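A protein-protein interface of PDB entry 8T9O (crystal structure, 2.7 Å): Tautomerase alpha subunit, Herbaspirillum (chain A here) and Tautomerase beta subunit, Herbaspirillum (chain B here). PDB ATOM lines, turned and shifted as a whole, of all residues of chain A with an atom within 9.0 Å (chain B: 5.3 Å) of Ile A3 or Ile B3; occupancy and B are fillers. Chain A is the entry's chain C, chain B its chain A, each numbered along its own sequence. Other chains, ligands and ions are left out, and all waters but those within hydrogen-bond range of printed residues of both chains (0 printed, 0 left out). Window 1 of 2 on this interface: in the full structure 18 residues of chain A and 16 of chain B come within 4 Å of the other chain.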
ATOM      1  N   PRO A   1      15.922   0.450  13.597  1.00  0.00           N
ATOM      2  CA  PRO A   1      14.853   0.378  14.594  1.00  0.00           C
ATOM      3  C   PRO A   1      14.043   1.669  14.647  1.00  0.00           C
ATOM      4  O   PRO A   1      14.385   2.630  13.959  1.00  0.00           O
ATOM      5  CB  PRO A   1      15.613   0.152  15.896  1.00  0.00           C
ATOM      6  CG  PRO A   1      16.843  -0.606  15.480  1.00  0.00           C
ATOM      7  CD  PRO A   1      17.133  -0.256  14.034  1.00  0.00           C
ATOM      8  N   ASN A   2      12.987   1.689  15.457  1.00  0.00           N
ATOM      9  CA  ASN A   2      12.146   2.868  15.593  1.00  0.00           C
ATOM     10  C   ASN A   2      11.690   2.997  17.037  1.00  0.00           C
ATOM     11  O   ASN A   2      11.218   2.024  17.631  1.00  0.00           O
ATOM     12  CB  ASN A   2      10.935   2.804  14.654  1.00  0.00           C
ATOM     13  CG  ASN A   2      11.326   2.868  13.186  1.00  0.00           C
ATOM     14  OD1 ASN A   2      11.841   3.880  12.714  1.00  0.00           O
ATOM     15  ND2 ASN A   2      11.072   1.787  12.458  1.00  0.00           N
ATOM     16  N   ILE A   3      11.829   4.200  17.592  1.00  0.00           N
ATOM     17  CA  ILE A   3      11.478   4.484  18.978  1.00  0.00           C
ATOM     18  C   ILE A   3      10.445   5.600  18.998  1.00  0.00           C
ATOM     19  O   ILE A   3      10.653   6.660  18.396  1.00  0.00           O
ATOM     20  CB  ILE A   3      12.714   4.877  19.810  1.00  0.00           C
ATOM     21  CG1 ILE A   3      13.702   3.714  19.902  1.00  0.00           C
ATOM     22  CG2 ILE A   3      12.301   5.333  21.201  1.00  0.00           C
ATOM     23  CD1 ILE A   3      15.050   4.113  20.473  1.00  0.00           C
ATOM     24  N   GLU A   4       9.333   5.355  19.682  1.00  0.00           N
ATOM     25  CA  GLU A   4       8.337   6.373  20.004  1.00  0.00           C
ATOM     26  C   GLU A   4       8.316   6.502  21.519  1.00  0.00           C
ATOM     27  O   GLU A   4       7.817   5.606  22.204  1.00  0.00           O
ATOM     28  CB  GLU A   4       6.958   5.990  19.478  1.00  0.00           C
ATOM     29  CG  GLU A   4       5.858   6.964  19.880  1.00  0.00           C
ATOM     30  CD  GLU A   4       4.511   6.595  19.299  1.00  0.00           C
ATOM     31  OE1 GLU A   4       4.238   5.384  19.165  1.00  0.00           O
ATOM     32  OE2 GLU A   4       3.728   7.512  18.978  1.00  0.00           O
ATOM     33  N   MET A   5       8.842   7.604  22.055  1.00  0.00           N
ATOM     34  CA  MET A   5       8.817   7.817  23.498  1.00  0.00           C
ATOM     35  C   MET A   5       7.692   8.772  23.875  1.00  0.00           C
ATOM     36  O   MET A   5       7.630   9.900  23.379  1.00  0.00           O
ATOM     37  CB  MET A   5      10.144   8.337  24.050  1.00  0.00           C
ATOM     38  CG  MET A   5      10.076   8.290  25.567  1.00  0.00           C
ATOM     39  SD  MET A   5      11.546   8.685  26.513  1.00  0.00           S
ATOM     40  CE  MET A   5      10.875   8.524  28.164  1.00  0.00           C
ATOM     41  N   PHE A   6       6.825   8.314  24.769  1.00  0.00           N
ATOM     42  CA  PHE A   6       5.737   9.121  25.290  1.00  0.00           C
ATOM     43  C   PHE A   6       6.220   9.877  26.520  1.00  0.00           C
ATOM     44  O   PHE A   6       6.597   9.263  27.524  1.00  0.00           O
ATOM     45  CB  PHE A   6       4.543   8.238  25.640  1.00  0.00           C
ATOM     46  CG  PHE A   6       3.933   7.549  24.460  1.00  0.00           C
ATOM     47  CD1 PHE A   6       2.952   8.171  23.710  1.00  0.00           C
ATOM     48  CD2 PHE A   6       4.349   6.281  24.095  1.00  0.00           C
ATOM     49  CE1 PHE A   6       2.385   7.537  22.625  1.00  0.00           C
ATOM     50  CE2 PHE A   6       3.787   5.639  23.010  1.00  0.00           C
ATOM     51  CZ  PHE A   6       2.803   6.269  22.274  1.00  0.00           C
ATOM     52  N   VAL A   7       6.215  11.208  26.441  1.00  0.00           N
ATOM     53  CA  VAL A   7       6.687  12.051  27.529  1.00  0.00           C
ATOM     54  C   VAL A   7       5.619  13.082  27.862  1.00  0.00           C
ATOM     55  O   VAL A   7       4.792  13.457  27.025  1.00  0.00           O
ATOM     56  CB  VAL A   7       8.021  12.744  27.188  1.00  0.00           C
ATOM     57  CG1 VAL A   7       9.136  11.719  27.083  1.00  0.00           C
ATOM     58  CG2 VAL A   7       7.890  13.525  25.892  1.00  0.00           C
ATOM     59  N   LEU A  19      17.848  13.968  24.557  1.00  0.00           N
ATOM     60  CA  LEU A  19      17.175  12.693  24.783  1.00  0.00           C
ATOM     61  C   LEU A  19      17.167  11.816  23.539  1.00  0.00           C
ATOM     62  O   LEU A  19      17.344  10.597  23.639  1.00  0.00           O
ATOM     63  CB  LEU A  19      15.742  12.936  25.258  1.00  0.00           C
ATOM     64  CG  LEU A  19      14.997  11.715  25.798  1.00  0.00           C
ATOM     65  CD1 LEU A  19      15.740  11.126  26.986  1.00  0.00           C
ATOM     66  CD2 LEU A  19      13.577  12.091  26.179  1.00  0.00           C
ATOM     67  N   ILE A  20      16.948  12.418  22.368  1.00  0.00           N
ATOM     68  CA  ILE A  20      17.058  11.676  21.115  1.00  0.00           C
ATOM     69  C   ILE A  20      18.458  11.095  20.966  1.00  0.00           C
ATOM     70  O   ILE A  20      18.629   9.953  20.525  1.00  0.00           O
ATOM     71  CB  ILE A  20      16.679  12.581  19.926  1.00  0.00           C
ATOM     72  CG1 ILE A  20      15.167  12.810  19.902  1.00  0.00           C
ATOM     73  CG2 ILE A  20      17.180  11.997  18.609  1.00  0.00           C
ATOM     74  CD1 ILE A  20      14.728  13.878  18.935  1.00  0.00           C
ATOM     75  N   ASP A  21      19.477  11.867  21.346  1.00  0.00           N
ATOM     76  CA  ASP A  21      20.845  11.355  21.358  1.00  0.00           C
ATOM     77  C   ASP A  21      20.984  10.184  22.323  1.00  0.00           C
ATOM     78  O   ASP A  21      21.468   9.110  21.949  1.00  0.00           O
ATOM     79  CB  ASP A  21      21.817  12.475  21.738  1.00  0.00           C
ATOM     80  CG  ASP A  21      23.271  12.054  21.621  1.00  0.00           C
ATOM     81  OD1 ASP A  21      23.801  11.476  22.592  1.00  0.00           O
ATOM     82  OD2 ASP A  21      23.883  12.310  20.563  1.00  0.00           O
ATOM     83  N   ALA A  22      20.557  10.377  23.574  1.00  0.00           N
ATOM     84  CA  ALA A  22      20.701   9.339  24.590  1.00  0.00           C
ATOM     85  C   ALA A  22      20.007   8.051  24.168  1.00  0.00           C
ATOM     86  O   ALA A  22      20.592   6.965  24.243  1.00  0.00           O
ATOM     87  CB  ALA A  22      20.146   9.839  25.924  1.00  0.00           C
ATOM     88  N   LEU A  23      18.754   8.154  23.716  1.00  0.00           N
ATOM     89  CA  LEU A  23      18.017   6.970  23.283  1.00  0.00           C
ATOM     90  C   LEU A  23      18.705   6.303  22.097  1.00  0.00           C
ATOM     91  O   LEU A  23      18.876   5.078  22.074  1.00  0.00           O
ATOM     92  CB  LEU A  23      16.579   7.349  22.925  1.00  0.00           C
ATOM     93  CG  LEU A  23      15.648   7.809  24.051  1.00  0.00           C
ATOM     94  CD1 LEU A  23      14.369   8.388  23.465  1.00  0.00           C
ATOM     95  CD2 LEU A  23      15.331   6.672  25.009  1.00  0.00           C
ATOM     96  N   THR A  24      19.104   7.098  21.097  1.00  0.00           N
ATOM     97  CA  THR A  24      19.835   6.554  19.956  1.00  0.00           C
ATOM     98  C   THR A  24      21.097   5.830  20.405  1.00  0.00           C
ATOM     99  O   THR A  24      21.408   4.740  19.912  1.00  0.00           O
ATOM    100  CB  THR A  24      20.190   7.672  18.973  1.00  0.00           C
ATOM    101  OG1 THR A  24      18.995   8.344  18.548  1.00  0.00           O
ATOM    102  CG2 THR A  24      20.919   7.112  17.761  1.00  0.00           C
ATOM    103  N   ALA A  25      21.832   6.418  21.352  1.00  0.00           N
ATOM    104  CA  ALA A  25      23.061   5.796  21.833  1.00  0.00           C
ATOM    105  C   ALA A  25      22.787   4.503  22.591  1.00  0.00           C
ATOM    106  O   ALA A  25      23.583   3.562  22.511  1.00  0.00           O
ATOM    107  CB  ALA A  25      23.832   6.778  22.714  1.00  0.00           C
ATOM    108  N   ALA A  26      21.674   4.436  23.329  1.00  0.00           N
ATOM    109  CA  ALA A  26      21.350   3.220  24.069  1.00  0.00           C
ATOM    110  C   ALA A  26      21.107   2.050  23.125  1.00  0.00           C
ATOM    111  O   ALA A  26      21.589   0.937  23.367  1.00  0.00           O
ATOM    112  CB  ALA A  26      20.129   3.456  24.957  1.00  0.00           C
ATOM    113  N   THR A  27      20.358   2.282  22.047  1.00  0.00           N
ATOM    114  CA  THR A  27      20.099   1.227  21.074  1.00  0.00           C
ATOM    115  C   THR A  27      21.373   0.790  20.366  1.00  0.00           C
ATOM    116  O   THR A  27      21.490  -0.373  19.965  1.00  0.00           O
ATOM    117  CB  THR A  27      19.073   1.701  20.047  1.00  0.00           C
ATOM    118  OG1 THR A  27      18.031   2.425  20.715  1.00  0.00           O
ATOM    119  CG2 THR A  27      18.469   0.524  19.304  1.00  0.00           C
ATOM    120  N   VAL A  28      22.328   1.705  20.202  1.00  0.00           N
ATOM    121  CA  VAL A  28      23.563   1.396  19.497  1.00  0.00           C
ATOM    122  C   VAL A  28      24.428   0.443  20.288  1.00  0.00           C
ATOM    123  O   VAL A  28      25.328  -0.206  19.735  1.00  0.00           O
ATOM    124  CB  VAL A  28      24.293   2.711  19.161  1.00  0.00           C
ATOM    125  CG1 VAL A  28      25.789   2.483  18.895  1.00  0.00           C
ATOM    126  CG2 VAL A  28      23.647   3.374  17.993  1.00  0.00           C
ATOM    127  N   SER A  37      20.463   4.195  11.336  1.00  0.00           N
ATOM    128  CA  SER A  37      19.283   3.383  11.076  1.00  0.00           C
ATOM    129  C   SER A  37      18.241   3.491  12.181  1.00  0.00           C
ATOM    130  O   SER A  37      17.274   2.726  12.180  1.00  0.00           O
ATOM    131  CB  SER A  37      19.688   1.922  10.881  1.00  0.00           C
ATOM    132  OG  SER A  37      19.954   1.298  12.127  1.00  0.00           O
ATOM    133  N   ILE A  38      18.407   4.427  13.111  1.00  0.00           N
ATOM    134  CA  ILE A  38      17.529   4.557  14.269  1.00  0.00           C
ATOM    135  C   ILE A  38      16.757   5.865  14.157  1.00  0.00           C
ATOM    136  O   ILE A  38      17.352   6.951  14.159  1.00  0.00           O
ATOM    137  CB  ILE A  38      18.318   4.480  15.585  1.00  0.00           C
ATOM    138  CG1 ILE A  38      19.141   3.190  15.625  1.00  0.00           C
ATOM    139  CG2 ILE A  38      17.387   4.579  16.780  1.00  0.00           C
ATOM    140  CD1 ILE A  38      20.244   3.201  16.649  1.00  0.00           C
ATOM    141  N   ARG A  39      15.433   5.755  14.061  1.00  0.00           N
ATOM    142  CA  ARG A  39      14.524   6.895  14.001  1.00  0.00           C
ATOM    143  C   ARG A  39      13.813   7.024  15.343  1.00  0.00           C
ATOM    144  O   ARG A  39      13.138   6.087  15.781  1.00  0.00           O
ATOM    145  CB  ARG A  39      13.503   6.725  12.875  1.00  0.00           C
ATOM    146  CG  ARG A  39      14.060   6.744  11.458  1.00  0.00           C
ATOM    147  CD  ARG A  39      12.901   6.640  10.475  1.00  0.00           C
ATOM    148  NE  ARG A  39      13.295   6.743   9.073  1.00  0.00           N
ATOM    149  CZ  ARG A  39      12.436   6.661   8.060  1.00  0.00           C
ATOM    150  NH1 ARG A  39      11.145   6.473   8.299  1.00  0.00           N
ATOM    151  NH2 ARG A  39      12.866   6.764   6.809  1.00  0.00           N
ATOM    152  N   VAL A  40      13.951   8.185  15.976  1.00  0.00           N
ATOM    153  CA  VAL A  40      13.445   8.432  17.324  1.00  0.00           C
ATOM    154  C   VAL A  40      12.455   9.586  17.257  1.00  0.00           C
ATOM    155  O   VAL A  40      12.800  10.672  16.779  1.00  0.00           O
ATOM    156  CB  VAL A  40      14.587   8.765  18.299  1.00  0.00           C
ATOM    157  CG1 VAL A  40      14.040   9.119  19.674  1.00  0.00           C
ATOM    158  CG2 VAL A  40      15.585   7.619  18.374  1.00  0.00           C
ATOM    159  N   TRP A  41      11.233   9.366  17.741  1.00  0.00           N
ATOM    160  CA  TRP A  41      10.286  10.469  17.847  1.00  0.00           C
ATOM    161  C   TRP A  41       9.670  10.542  19.234  1.00  0.00           C
ATOM    162  O   TRP A  41       9.396   9.521  19.871  1.00  0.00           O
ATOM    163  CB  TRP A  41       9.177  10.417  16.776  1.00  0.00           C
ATOM    164  CG  TRP A  41       8.399   9.145  16.635  1.00  0.00           C
ATOM    165  CD1 TRP A  41       7.191   8.850  17.201  1.00  0.00           C
ATOM    166  CD2 TRP A  41       8.744   8.024  15.818  1.00  0.00           C
ATOM    167  NE1 TRP A  41       6.778   7.603  16.802  1.00  0.00           N
ATOM    168  CE2 TRP A  41       7.715   7.073  15.955  1.00  0.00           C
ATOM    169  CE3 TRP A  41       9.832   7.728  14.994  1.00  0.00           C
ATOM    170  CZ2 TRP A  41       7.743   5.845  15.302  1.00  0.00           C
ATOM    171  CZ3 TRP A  41       9.859   6.509  14.345  1.00  0.00           C
ATOM    172  CH2 TRP A  41       8.820   5.583  14.501  1.00  0.00           C
ATOM    173  N   LEU A  42       9.469  11.776  19.682  1.00  0.00           N
ATOM    174  CA  LEU A  42       8.891  12.092  20.978  1.00  0.00           C
ATOM    175  C   LEU A  42       7.434  12.490  20.787  1.00  0.00           C
ATOM    176  O   LEU A  42       7.139  13.440  20.053  1.00  0.00           O
ATOM    177  CB  LEU A  42       9.689  13.213  21.644  1.00  0.00           C
ATOM    178  CG  LEU A  42      11.073  12.749  22.088  1.00  0.00           C
ATOM    179  CD1 LEU A  42      11.832  13.872  22.762  1.00  0.00           C
ATOM    180  CD2 LEU A  42      10.900  11.603  23.054  1.00  0.00           C
ATOM    181  N   SER A  43       6.532  11.753  21.424  1.00  0.00           N
ATOM    182  CA  SER A  43       5.104  12.046  21.379  1.00  0.00           C
ATOM    183  C   SER A  43       4.735  12.721  22.694  1.00  0.00           C
ATOM    184  O   SER A  43       4.497  12.057  23.707  1.00  0.00           O
ATOM    185  CB  SER A  43       4.292  10.782  21.128  1.00  0.00           C
ATOM    186  OG  SER A  43       4.515  10.305  19.812  1.00  0.00           O
ATOM    187  N   PHE A  50      -2.365  12.434  30.382  1.00  0.00           N
ATOM    188  CA  PHE A  50      -1.457  11.349  30.750  1.00  0.00           C
ATOM    189  C   PHE A  50      -1.933  10.770  32.076  1.00  0.00           C
ATOM    190  O   PHE A  50      -1.834  11.430  33.116  1.00  0.00           O
ATOM    191  CB  PHE A  50      -0.015  11.849  30.841  1.00  0.00           C
ATOM    192  CG  PHE A  50       1.021  10.774  30.635  1.00  0.00           C
ATOM    193  CD1 PHE A  50       1.234   9.804  31.602  1.00  0.00           C
ATOM    194  CD2 PHE A  50       1.789  10.741  29.481  1.00  0.00           C
ATOM    195  CE1 PHE A  50       2.188   8.817  31.419  1.00  0.00           C
ATOM    196  CE2 PHE A  50       2.745   9.757  29.293  1.00  0.00           C
ATOM    197  CZ  PHE A  50       2.943   8.794  30.264  1.00  0.00           C
ATOM    198  N   SER B   1       8.103   8.451  29.951  1.00  0.00           N
ATOM    199  CA  SER B   1       7.731   7.371  30.852  1.00  0.00           C
ATOM    200  C   SER B   1       7.457   6.054  30.117  1.00  0.00           C
ATOM    201  O   SER B   1       7.630   4.981  30.688  1.00  0.00           O
ATOM    202  CB  SER B   1       6.513   7.772  31.688  1.00  0.00           C
ATOM    203  OG  SER B   1       6.685   9.066  32.245  1.00  0.00           O
ATOM    204  N   ILE B   2       7.031   6.127  28.857  1.00  0.00           N
ATOM    205  CA  ILE B   2       6.727   4.933  28.071  1.00  0.00           C
ATOM    206  C   ILE B   2       7.517   4.981  26.770  1.00  0.00           C
ATOM    207  O   ILE B   2       7.365   5.917  25.976  1.00  0.00           O
ATOM    208  CB  ILE B   2       5.220   4.781  27.810  1.00  0.00           C
ATOM    209  CG1 ILE B   2       4.433   5.138  29.073  1.00  0.00           C
ATOM    210  CG2 ILE B   2       4.892   3.366  27.363  1.00  0.00           C
ATOM    211  CD1 ILE B   2       2.953   5.225  28.881  1.00  0.00           C
ATOM    212  N   ILE B   3       8.357   3.969  26.560  1.00  0.00           N
ATOM    213  CA  ILE B   3       9.189   3.839  25.368  1.00  0.00           C
ATOM    214  C   ILE B   3       8.683   2.643  24.574  1.00  0.00           C
ATOM    215  O   ILE B   3       8.625   1.522  25.095  1.00  0.00           O
ATOM    216  CB  ILE B   3      10.673   3.668  25.727  1.00  0.00           C
ATOM    217  CG1 ILE B   3      11.177   4.856  26.549  1.00  0.00           C
ATOM    218  CG2 ILE B   3      11.511   3.494  24.469  1.00  0.00           C
ATOM    219  CD1 ILE B   3      12.456   4.565  27.307  1.00  0.00           C
ATOM    220  N   GLN B   4       8.321   2.878  23.317  1.00  0.00           N
ATOM    221  CA  GLN B   4       7.850   1.840  22.409  1.00  0.00           C
ATOM    222  C   GLN B   4       8.873   1.648  21.299  1.00  0.00           C
ATOM    223  O   GLN B   4       9.273   2.619  20.649  1.00  0.00           O
ATOM    224  CB  GLN B   4       6.490   2.219  21.818  1.00  0.00           C
ATOM    225  CG  GLN B   4       5.701   1.060  21.230  1.00  0.00           C
ATOM    226  CD  GLN B   4       4.438   1.527  20.528  1.00  0.00           C
ATOM    227  OE1 GLN B   4       3.681   0.723  19.985  1.00  0.00           O
ATOM    228  NE2 GLN B   4       4.212   2.836  20.525  1.00  0.00           N
ATOM    229  N   VAL B   5       9.292   0.403  21.081  1.00  0.00           N
ATOM    230  CA  VAL B   5      10.303   0.075  20.079  1.00  0.00           C
ATOM    231  C   VAL B   5       9.668  -0.800  19.005  1.00  0.00           C
ATOM    232  O   VAL B   5       9.107  -1.863  19.307  1.00  0.00           O
ATOM    233  CB  VAL B   5      11.523  -0.617  20.706  1.00  0.00           C
ATOM    234  CG1 VAL B   5      12.517  -1.017  19.628  1.00  0.00           C
ATOM    235  CG2 VAL B   5      12.188   0.299  21.726  1.00  0.00           C
ATOM    236  N   PHE B   6       9.757  -0.346  17.753  1.00  0.00           N
ATOM    237  CA  PHE B   6       9.329  -1.093  16.577  1.00  0.00           C
ATOM    238  C   PHE B   6      10.581  -1.551  15.847  1.00  0.00           C
ATOM    239  O   PHE B   6      11.386  -0.713  15.429  1.00  0.00           O
ATOM    240  CB  PHE B   6       8.503  -0.225  15.629  1.00  0.00           C
ATOM    241  CG  PHE B   6       7.415   0.563  16.284  1.00  0.00           C
ATOM    242  CD1 PHE B   6       6.181  -0.002  16.551  1.00  0.00           C
ATOM    243  CD2 PHE B   6       7.624   1.895  16.608  1.00  0.00           C
ATOM    244  CE1 PHE B   6       5.178   0.745  17.141  1.00  0.00           C
ATOM    245  CE2 PHE B   6       6.629   2.644  17.200  1.00  0.00           C
ATOM    246  CZ  PHE B   6       5.405   2.069  17.464  1.00  0.00           C
ATOM    247  N   LEU B  23      17.494   1.614  27.600  1.00  0.00           N
ATOM    248  CA  LEU B  23      16.597   2.720  27.300  1.00  0.00           C
ATOM    249  C   LEU B  23      16.034   3.355  28.564  1.00  0.00           C
ATOM    250  O   LEU B  23      15.880   4.582  28.620  1.00  0.00           O
ATOM    251  CB  LEU B  23      15.453   2.234  26.411  1.00  0.00           C
ATOM    252  CG  LEU B  23      15.842   1.850  24.980  1.00  0.00           C
ATOM    253  CD1 LEU B  23      14.726   1.055  24.318  1.00  0.00           C
ATOM    254  CD2 LEU B  23      16.202   3.077  24.156  1.00  0.00           C
ATOM    255  N   THR B  24      15.700   2.537  29.563  1.00  0.00           N
ATOM    256  CA  THR B  24      15.284   3.058  30.861  1.00  0.00           C
ATOM    257  C   THR B  24      16.338   3.979  31.439  1.00  0.00           C
ATOM    258  O   THR B  24      16.025   5.033  32.002  1.00  0.00           O
ATOM    259  CB  THR B  24      15.037   1.902  31.825  1.00  0.00           C
ATOM    260  OG1 THR B  24      14.159   0.949  31.217  1.00  0.00           O
ATOM    261  CG2 THR B  24      14.456   2.403  33.145  1.00  0.00           C
ATOM    262  N   ALA B  27      16.476   7.485  29.804  1.00  0.00           N
ATOM    263  CA  ALA B  27      15.482   8.443  30.286  1.00  0.00           C
ATOM    264  C   ALA B  27      15.808   8.914  31.698  1.00  0.00           C
ATOM    265  O   ALA B  27      15.721  10.112  31.996  1.00  0.00           O
ATOM    266  CB  ALA B  27      14.084   7.826  30.238  1.00  0.00           C
ATOM    267  N   VAL B  38       9.036   3.952  34.299  1.00  0.00           N
ATOM    268  CA  VAL B  38       9.483   3.723  32.931  1.00  0.00           C
ATOM    269  C   VAL B  38       8.924   2.395  32.445  1.00  0.00           C
ATOM    270  O   VAL B  38       9.069   1.363  33.111  1.00  0.00           O
ATOM    271  CB  VAL B  38      11.015   3.743  32.823  1.00  0.00           C
ATOM    272  CG1 VAL B  38      11.441   3.043  31.542  1.00  0.00           C
ATOM    273  CG2 VAL B  38      11.533   5.171  32.850  1.00  0.00           C
ATOM    274  N   ARG B  39       8.282   2.426  31.281  1.00  0.00           N
ATOM    275  CA  ARG B  39       7.785   1.234  30.616  1.00  0.00           C
ATOM    276  C   ARG B  39       8.425   1.155  29.240  1.00  0.00           C
ATOM    277  O   ARG B  39       8.429   2.141  28.495  1.00  0.00           O
ATOM    278  CB  ARG B  39       6.261   1.262  30.523  1.00  0.00           C
ATOM    279  CG  ARG B  39       5.626   1.478  31.881  1.00  0.00           C
ATOM    280  CD  ARG B  39       5.830   0.250  32.749  1.00  0.00           C
ATOM    281  NE  ARG B  39       5.763   0.547  34.176  1.00  0.00           N
ATOM    282  CZ  ARG B  39       4.650   0.528  34.903  1.00  0.00           C
ATOM    283  NH1 ARG B  39       3.487   0.232  34.340  1.00  0.00           N
ATOM    284  NH2 ARG B  39       4.702   0.810  36.196  1.00  0.00           N
ATOM    285  N   VAL B  40       8.991  -0.004  28.920  1.00  0.00           N
ATOM    286  CA  VAL B  40       9.655  -0.241  27.645  1.00  0.00           C
ATOM    287  C   VAL B  40       8.920  -1.376  26.951  1.00  0.00           C
ATOM    288  O   VAL B  40       8.921  -2.516  27.436  1.00  0.00           O
ATOM    289  CB  VAL B  40      11.144  -0.568  27.814  1.00  0.00           C
ATOM    290  CG1 VAL B  40      11.831  -0.612  26.460  1.00  0.00           C
ATOM    291  CG2 VAL B  40      11.811   0.462  28.709  1.00  0.00           C
ATOM    292  N   ILE B  41       8.301  -1.071  25.816  1.00  0.00           N
ATOM    293  CA  ILE B  41       7.487  -2.030  25.080  1.00  0.00           C
ATOM    294  C   ILE B  41       8.246  -2.348  23.798  1.00  0.00           C
ATOM    295  O   ILE B  41       8.515  -1.447  22.993  1.00  0.00           O
ATOM    296  CB  ILE B  41       6.100  -1.459  24.758  1.00  0.00           C
ATOM    297  CG1 ILE B  41       5.411  -0.938  26.012  1.00  0.00           C
ATOM    298  CG2 ILE B  41       5.203  -2.568  24.250  1.00  0.00           C
ATOM    299  CD1 ILE B  41       4.180  -0.102  25.691  1.00  0.00           C
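Val B5 touches Asn A2.
Gln B4 touches Ile A3 (O to CA, 3.3 Å).
Ile B2 touches Glu A4.
Ile B3 touches Glu A4.
Phe B6 touches Glu A4 (CZ to OE1, 3.9 Å).
Ser B1 touches Met A5 (N to CE, 3.3 Å).
Ile B2 touches Met A5.
Met A5 touches Ile B3 (CG to CG1, 3.7 Å).
Leu B23 touches Leu A23 (CD2 to CD2, 3.8 Å).
Ile B2 touches Phe A50.
Printed residues of chain B within 4 Å of Pro A1: Phe B6.
Of the printed residues of chain B, Ile A3 touches Ile B3, Gln B4 and Leu B23.
Printed residues of chain A within 4 Å of Ser B1: Met A5 (3.3 Å), Phe A6 (3.0 Å) and Phe A50 (3.98 Å).
Of the printed residues of chain A, Ile B2 touches Glu A4, Met A5, Phe A6 and Phe A50.
Of the printed residues of chain A, Ile B3 touches Ile A3, Glu A4 and Met A5.
Of the printed residues of chain A, Val B5 touches Asn A2 (3.3 Å).
Thr B24 touches none of the printed residues of chain A.
No residue of chain A comes within 4 Å of Val B40.
The nearest printed residue of chain B that does not touch Ile A3 is Val B5 (4.2 Å).
The nearest printed residue of chain B that does not touch Met A5 is Gln B4 (4.9 Å).
The side-chain carboxylate (OE2) of Glu A4 is in hydrogen-bond range of the side-chain hydroxyl (OG) of Ser A43 (3.0 Å).
O of Ile B3 is in hydrogen-bond range of N of Ile B41, at 2.7 Å.
O of Arg B39 is in hydrogen-bond range of N of Ile B3 (2.7 Å).
O of Leu A23 is in hydrogen-bond range of OG1 of Thr A27.
The backbone NH of Met A5 lies within hydrogen-bond range of the backbone carbonyl oxygen of Trp A41 (3.0 Å).
O of Ile A3 is in hydrogen-bond range of N of Trp A41.
Printed residues of chain B that touch a printed residue of chain A: Ser B1, Ile B2, Ile B3, Gln B4, Val B5, Phe B6, Leu B23 and Ala B27.
Among the printed residues, 23 pairs touch across the chains.
Among the printed residues, no Asp or Glu carboxylate lies within 4 Å of a Lys or Arg side-chain nitrogen of the other chain.
The side-chain amide nitrogen (NE2) of Gln B4 is in hydrogen-bond range of the side-chain carboxylate (OE1) of Glu A4.
The backbone carbonyl oxygen of Ile B2 lies within hydrogen-bond range of the backbone NH of Phe A6.
The backbone carbonyl oxygen (O) of Phe A6 lies within hydrogen-bond range of the backbone NH (N) of Ser B1 (3.0 Å).
The backbone carbonyl oxygen (O) of Asn A2 lies within hydrogen-bond range of the backbone NH (N) of Phe B6, at 2.8 Å.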
